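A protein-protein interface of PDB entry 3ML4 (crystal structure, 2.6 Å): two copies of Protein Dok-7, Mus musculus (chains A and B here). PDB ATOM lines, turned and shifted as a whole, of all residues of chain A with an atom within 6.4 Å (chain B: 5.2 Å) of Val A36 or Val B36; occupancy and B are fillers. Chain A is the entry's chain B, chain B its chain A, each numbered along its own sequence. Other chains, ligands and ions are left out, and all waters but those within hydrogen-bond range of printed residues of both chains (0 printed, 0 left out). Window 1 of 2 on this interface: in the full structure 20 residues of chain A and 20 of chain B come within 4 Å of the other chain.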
ATOM      1  N   LYS A  32     -34.741  23.713  10.327  1.00  0.00           N
ATOM      2  CA  LYS A  32     -34.066  23.790  11.618  1.00  0.00           C
ATOM      3  C   LYS A  32     -34.899  24.653  12.565  1.00  0.00           C
ATOM      4  O   LYS A  32     -35.273  25.769  12.201  1.00  0.00           O
ATOM      5  CB  LYS A  32     -32.666  24.384  11.447  1.00  0.00           C
ATOM      6  CG  LYS A  32     -31.681  23.470  10.723  1.00  0.00           C
ATOM      7  CD  LYS A  32     -30.489  24.239  10.161  1.00  0.00           C
ATOM      8  CE  LYS A  32     -29.328  24.342  11.152  1.00  0.00           C
ATOM      9  NZ  LYS A  32     -29.540  25.379  12.195  1.00  0.00           N
ATOM     10  N   SER A  34     -34.006  26.173  15.196  1.00  0.00           N
ATOM     11  CA  SER A  34     -33.228  27.345  15.564  1.00  0.00           C
ATOM     12  C   SER A  34     -32.001  27.454  14.662  1.00  0.00           C
ATOM     13  O   SER A  34     -31.599  26.457  14.054  1.00  0.00           O
ATOM     14  CB  SER A  34     -32.817  27.266  17.033  1.00  0.00           C
ATOM     15  OG  SER A  34     -31.989  26.146  17.286  1.00  0.00           O
ATOM     16  N   PRO A  35     -31.400  28.660  14.570  1.00  0.00           N
ATOM     17  CA  PRO A  35     -30.264  28.913  13.663  1.00  0.00           C
ATOM     18  C   PRO A  35     -29.010  28.079  13.935  1.00  0.00           C
ATOM     19  O   PRO A  35     -28.118  28.015  13.086  1.00  0.00           O
ATOM     20  CB  PRO A  35     -29.956  30.401  13.878  1.00  0.00           C
ATOM     21  CG  PRO A  35     -30.607  30.764  15.152  1.00  0.00           C
ATOM     22  CD  PRO A  35     -31.785  29.873  15.315  1.00  0.00           C
ATOM     23  N   VAL A  36     -28.955  27.447  15.102  1.00  0.00           N
ATOM     24  CA  VAL A  36     -27.797  26.666  15.516  1.00  0.00           C
ATOM     25  C   VAL A  36     -28.290  25.296  16.008  1.00  0.00           C
ATOM     26  O   VAL A  36     -27.910  24.809  17.076  1.00  0.00           O
ATOM     27  CB  VAL A  36     -26.952  27.476  16.563  1.00  0.00           C
ATOM     28  CG1 VAL A  36     -26.122  26.582  17.469  1.00  0.00           C
ATOM     29  CG2 VAL A  36     -26.055  28.495  15.850  1.00  0.00           C
ATOM     30  N   ALA A  37     -29.135  24.667  15.197  1.00  0.00           N
ATOM     31  CA  ALA A  37     -29.806  23.437  15.606  1.00  0.00           C
ATOM     32  C   ALA A  37     -29.195  22.165  15.025  1.00  0.00           C
ATOM     33  O   ALA A  37     -28.867  22.102  13.840  1.00  0.00           O
ATOM     34  CB  ALA A  37     -31.295  23.512  15.277  1.00  0.00           C
ATOM     35  N   ASP A  38     -29.037  21.163  15.888  1.00  0.00           N
ATOM     36  CA  ASP A  38     -28.741  19.792  15.483  1.00  0.00           C
ATOM     37  C   ASP A  38     -30.053  19.070  15.173  1.00  0.00           C
ATOM     38  O   ASP A  38     -30.058  17.920  14.725  1.00  0.00           O
ATOM     39  CB  ASP A  38     -27.998  19.050  16.603  1.00  0.00           C
ATOM     40  CG  ASP A  38     -26.488  19.193  16.503  1.00  0.00           C
ATOM     41  OD1 ASP A  38     -25.933  18.907  15.419  1.00  0.00           O
ATOM     42  OD2 ASP A  38     -25.852  19.581  17.508  1.00  0.00           O
ATOM     43  N   CYS A  39     -31.160  19.765  15.422  1.00  0.00           N
ATOM     44  CA  CYS A  39     -32.492  19.195  15.284  1.00  0.00           C
ATOM     45  C   CYS A  39     -33.116  19.515  13.936  1.00  0.00           C
ATOM     46  O   CYS A  39     -32.666  20.411  13.221  1.00  0.00           O
ATOM     47  CB  CYS A  39     -33.411  19.720  16.392  1.00  0.00           C
ATOM     48  SG  CYS A  39     -32.685  19.702  18.035  1.00  0.00           S
ATOM     49  N   ALA A 111     -26.804  21.731   5.863  1.00  0.00           N
ATOM     50  CA  ALA A 111     -27.539  22.501   6.862  1.00  0.00           C
ATOM     51  C   ALA A 111     -27.262  22.075   8.302  1.00  0.00           C
ATOM     52  O   ALA A 111     -27.240  22.915   9.200  1.00  0.00           O
ATOM     53  CB  ALA A 111     -29.018  22.445   6.576  1.00  0.00           C
ATOM     54  N   LEU A 112     -27.049  20.777   8.519  1.00  0.00           N
ATOM     55  CA  LEU A 112     -26.839  20.258   9.879  1.00  0.00           C
ATOM     56  C   LEU A 112     -25.421  20.478  10.427  1.00  0.00           C
ATOM     57  O   LEU A 112     -25.175  20.275  11.618  1.00  0.00           O
ATOM     58  CB  LEU A 112     -27.259  18.790   9.990  1.00  0.00           C
ATOM     59  CG  LEU A 112     -28.761  18.501   9.860  1.00  0.00           C
ATOM     60  CD1 LEU A 112     -29.027  16.995   9.861  1.00  0.00           C
ATOM     61  CD2 LEU A 112     -29.591  19.209  10.947  1.00  0.00           C
ATOM     62  N   GLY A 113     -24.501  20.901   9.560  1.00  0.00           N
ATOM     63  CA  GLY A 113     -23.139  21.239   9.975  1.00  0.00           C
ATOM     64  C   GLY A 113     -22.106  20.360   9.304  1.00  0.00           C
ATOM     65  O   GLY A 113     -21.829  20.511   8.110  1.00  0.00           O
ATOM     66  N   GLU A 114     -21.529  19.443  10.073  1.00  0.00           N
ATOM     67  CA  GLU A 114     -20.603  18.463   9.511  1.00  0.00           C
ATOM     68  C   GLU A 114     -21.159  17.056   9.698  1.00  0.00           C
ATOM     69  O   GLU A 114     -21.053  16.465  10.780  1.00  0.00           O
ATOM     70  CB  GLU A 114     -19.202  18.609  10.117  1.00  0.00           C
ATOM     71  CG  GLU A 114     -18.501  19.929   9.776  1.00  0.00           C
ATOM     72  CD  GLU A 114     -18.145  20.071   8.295  1.00  0.00           C
ATOM     73  OE1 GLU A 114     -17.931  19.048   7.603  1.00  0.00           O
ATOM     74  OE2 GLU A 114     -18.077  21.225   7.820  1.00  0.00           O
ATOM     75  N   ASN A 139     -21.249  16.072  13.599  1.00  0.00           N
ATOM     76  CA  ASN A 139     -20.629  17.135  14.394  1.00  0.00           C
ATOM     77  C   ASN A 139     -19.756  16.612  15.548  1.00  0.00           C
ATOM     78  O   ASN A 139     -18.602  16.253  15.341  1.00  0.00           O
ATOM     79  CB  ASN A 139     -21.671  18.159  14.884  1.00  0.00           C
ATOM     80  CG  ASN A 139     -22.470  18.778  13.746  1.00  0.00           C
ATOM     81  OD1 ASN A 139     -21.925  19.467  12.884  1.00  0.00           O
ATOM     82  ND2 ASN A 139     -23.773  18.539  13.746  1.00  0.00           N
ATOM     83  N   ASP A 140     -20.313  16.570  16.752  1.00  0.00           N
ATOM     84  CA  ASP A 140     -19.559  16.198  17.947  1.00  0.00           C
ATOM     85  C   ASP A 140     -19.661  14.706  18.296  1.00  0.00           C
ATOM     86  O   ASP A 140     -19.003  14.241  19.230  1.00  0.00           O
ATOM     87  CB  ASP A 140     -19.969  17.076  19.145  1.00  0.00           C
ATOM     88  CG  ASP A 140     -21.440  17.515  19.093  1.00  0.00           C
ATOM     89  OD1 ASP A 140     -21.760  18.600  19.637  1.00  0.00           O
ATOM     90  OD2 ASP A 140     -22.275  16.787  18.511  1.00  0.00           O
ATOM     91  N   PHE A 214     -15.067  26.975  12.676  1.00  0.00           N
ATOM     92  CA  PHE A 214     -16.495  27.092  12.982  1.00  0.00           C
ATOM     93  C   PHE A 214     -16.825  28.519  13.425  1.00  0.00           C
ATOM     94  O   PHE A 214     -17.980  28.941  13.380  1.00  0.00           O
ATOM     95  CB  PHE A 214     -16.936  26.097  14.071  1.00  0.00           C
ATOM     96  CG  PHE A 214     -16.517  24.663  13.827  1.00  0.00           C
ATOM     97  CD1 PHE A 214     -16.548  24.104  12.552  1.00  0.00           C
ATOM     98  CD2 PHE A 214     -16.129  23.857  14.895  1.00  0.00           C
ATOM     99  CE1 PHE A 214     -16.163  22.776  12.339  1.00  0.00           C
ATOM    100  CE2 PHE A 214     -15.750  22.529  14.696  1.00  0.00           C
ATOM    101  CZ  PHE A 214     -15.766  21.987  13.415  1.00  0.00           C
ATOM    102  N   LYS B  32     -15.525  27.601  18.578  1.00  0.00           N
ATOM    103  CA  LYS B  32     -16.622  26.682  18.832  1.00  0.00           C
ATOM    104  C   LYS B  32     -16.079  25.259  18.916  1.00  0.00           C
ATOM    105  O   LYS B  32     -15.227  24.880  18.112  1.00  0.00           O
ATOM    106  CB  LYS B  32     -17.658  26.764  17.709  1.00  0.00           C
ATOM    107  CG  LYS B  32     -18.614  27.945  17.788  1.00  0.00           C
ATOM    108  CD  LYS B  32     -19.343  28.115  16.469  1.00  0.00           C
ATOM    109  CE  LYS B  32     -20.728  28.696  16.656  1.00  0.00           C
ATOM    110  NZ  LYS B  32     -21.762  27.649  16.895  1.00  0.00           N
ATOM    111  N   SER B  34     -18.202  22.650  18.625  1.00  0.00           N
ATOM    112  CA  SER B  34     -19.057  22.008  17.629  1.00  0.00           C
ATOM    113  C   SER B  34     -19.511  23.032  16.591  1.00  0.00           C
ATOM    114  O   SER B  34     -19.866  24.157  16.951  1.00  0.00           O
ATOM    115  CB  SER B  34     -20.277  21.368  18.300  1.00  0.00           C
ATOM    116  OG  SER B  34     -21.344  21.185  17.375  1.00  0.00           O
ATOM    117  N   PRO B  35     -19.515  22.642  15.301  1.00  0.00           N
ATOM    118  CA  PRO B  35     -19.867  23.536  14.185  1.00  0.00           C
ATOM    119  C   PRO B  35     -21.254  24.156  14.298  1.00  0.00           C
ATOM    120  O   PRO B  35     -21.519  25.205  13.701  1.00  0.00           O
ATOM    121  CB  PRO B  35     -19.813  22.619  12.961  1.00  0.00           C
ATOM    122  CG  PRO B  35     -19.780  21.240  13.484  1.00  0.00           C
ATOM    123  CD  PRO B  35     -19.165  21.292  14.829  1.00  0.00           C
ATOM    124  N   VAL B  36     -22.124  23.501  15.059  1.00  0.00           N
ATOM    125  CA  VAL B  36     -23.493  23.944  15.263  1.00  0.00           C
ATOM    126  C   VAL B  36     -23.861  23.642  16.725  1.00  0.00           C
ATOM    127  O   VAL B  36     -24.530  22.646  17.028  1.00  0.00           O
ATOM    128  CB  VAL B  36     -24.469  23.281  14.228  1.00  0.00           C
ATOM    129  CG1 VAL B  36     -25.913  23.381  14.675  1.00  0.00           C
ATOM    130  CG2 VAL B  36     -24.316  23.917  12.843  1.00  0.00           C
ATOM    131  N   ALA B  37     -23.368  24.498  17.622  1.00  0.00           N
ATOM    132  CA  ALA B  37     -23.669  24.441  19.056  1.00  0.00           C
ATOM    133  C   ALA B  37     -23.398  25.797  19.710  1.00  0.00           C
ATOM    134  O   ALA B  37     -22.519  26.545  19.269  1.00  0.00           O
ATOM    135  CB  ALA B  37     -22.858  23.352  19.740  1.00  0.00           C
ATOM    136  N   ASP B  38     -24.155  26.102  20.762  1.00  0.00           N
ATOM    137  CA  ASP B  38     -24.031  27.369  21.482  1.00  0.00           C
ATOM    138  C   ASP B  38     -22.974  27.317  22.578  1.00  0.00           C
ATOM    139  O   ASP B  38     -23.288  27.457  23.766  1.00  0.00           O
ATOM    140  CB  ASP B  38     -25.381  27.781  22.077  1.00  0.00           C
ATOM    141  CG  ASP B  38     -26.131  28.754  21.197  1.00  0.00           C
ATOM    142  OD1 ASP B  38     -25.555  29.223  20.189  1.00  0.00           O
ATOM    143  OD2 ASP B  38     -27.301  29.057  21.519  1.00  0.00           O
ATOM    144  N   LEU B 112     -21.840  32.782  16.648  1.00  0.00           N
ATOM    145  CA  LEU B 112     -22.809  32.049  17.474  1.00  0.00           C
ATOM    146  C   LEU B 112     -24.222  31.970  16.871  1.00  0.00           C
ATOM    147  O   LEU B 112     -25.156  31.478  17.512  1.00  0.00           O
ATOM    148  CB  LEU B 112     -22.875  32.639  18.886  1.00  0.00           C
ATOM    149  CG  LEU B 112     -21.632  32.594  19.780  1.00  0.00           C
ATOM    150  CD1 LEU B 112     -21.904  33.407  21.042  1.00  0.00           C
ATOM    151  CD2 LEU B 112     -21.214  31.162  20.126  1.00  0.00           C
ATOM    152  N   GLY B 113     -24.373  32.456  15.645  1.00  0.00           N
ATOM    153  CA  GLY B 113     -25.650  32.395  14.958  1.00  0.00           C
ATOM    154  C   GLY B 113     -26.388  33.707  15.036  1.00  0.00           C
ATOM    155  O   GLY B 113     -25.950  34.704  14.464  1.00  0.00           O
ATOM    156  N   ASN B 139     -30.281  32.939  19.742  1.00  0.00           N
ATOM    157  CA  ASN B 139     -30.861  31.825  18.992  1.00  0.00           C
ATOM    158  C   ASN B 139     -32.214  31.395  19.553  1.00  0.00           C
ATOM    159  O   ASN B 139     -33.228  32.009  19.231  1.00  0.00           O
ATOM    160  CB  ASN B 139     -29.878  30.653  18.879  1.00  0.00           C
ATOM    161  CG  ASN B 139     -28.563  31.055  18.229  1.00  0.00           C
ATOM    162  OD1 ASN B 139     -28.549  31.712  17.190  1.00  0.00           O
ATOM    163  ND2 ASN B 139     -27.449  30.665  18.845  1.00  0.00           N
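The side-chain carboxylate (OD1) of Asp A140 sits close to the side-chain hydroxyl (OG) of Ser B34, at 3.5 Å. The backbone carbonyl oxygen (O) of Val B36 sits close to the side-chain carboxylate (OD2) of Asp A38 (3.4 Å).
OG of Ser B34 sits close to N of Val B36. The backbone carbonyl oxygen (O) of Pro A35 sits at hydrogen-bond distance from the side-chain amino group (NZ) of Lys A32, 3.1 Å away. The side-chain carboxylate (OD1) of Asp B38 sits at hydrogen-bond distance from the side-chain amide nitrogen (ND2) of Asn B139 (2.7 Å). N of Glu A114 sits at hydrogen-bond distance from OD1 of Asn A139 (2.8 Å). The backbone carbonyl oxygen of Leu A112 sits at hydrogen-bond distance from the side-chain amide nitrogen of Asn A139, at 3.1 Å. OD1 of Asp A38 is in hydrogen-bond range of ND2 of Asn A139 (2.8 Å).
Among the printed residues, merely in contact across the chains: Pro A35 with Asn B139 (3.0 Å), Val A36 with Val B36 (3.3 Å), Val A36 with Ala B37 (3.5 Å), Val A36 with Asp B38 (3.8 Å), Val A36 with Leu B112 (3.5 Å), Val A36 with Asn B139 (3.95 Å), Ala A37 with Val B36 (3.3 Å), Leu A112 with Val B36 (3.9 Å), Asn A139 with Ser B34 (3.9 Å), Asn A139 with Pro B35 (2.8 Å), Phe A214 with Lys B32 (3.5 Å), Phe A214 with Ser B34 (3.9 Å) and Phe A214 with Pro B35 (3.6 Å).
Val A36 touches five residues of chain B. Printed residues of chain B within 4 Å of Ala A37: Val B36 (3.3 Å). Glu A114 touches none of the printed residues of chain B. Of the printed residues of chain A, Pro B35 touches Asn A139 and Phe A214. Of chain A, only Val A36, Ala A37, Asp A38 and Leu A112 come within 4 Å of Val B36. Printed residues of chain A within 4 Å of Ala B37: Val A36 (3.5 Å). Of the printed residues of chain A, Leu B112 touches Val A36. Gly B113 touches none of the printed residues of chain A. Printed residues of chain A within 4 Å of Asn B139: Pro A35 (3.0 Å) and Val A36 (3.95 Å). The nearest residue of chain B that does not touch Val A36 is Gly B113 (4.02 Å). The nearest residue of chain A that does not touch Val B36 is Gly A113 (4.1 Å).
Of the 9 printed residues of chain B, 8 touch a printed residue of chain A. Hydrophobic or aromatic side chains of chain B that line the printed part of chain A: Pro B35 and Val B36. Among the printed residues, 15 pairs touch across the chains. Among the printed residues, no Asp or Glu carboxylate lies within 4 Å of a Lys or Arg side-chain nitrogen of the other chain.
Pro A35 touches Asn B139, and with the chains exchanged Asn A139 touches Pro B35. Val B36 touches its own counterpart, Val A36. Val A36 touches Ala B37, and with the chains exchanged Ala A37 touches Val B36. Val A36 touches Asp B38, and with the chains exchanged Asp A38 touches Val B36. 9 positions are printed for both chains. Of the 15 pairs that touch across the chains among the printed residues, 9 have their exchanged pair printed and touching as well.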
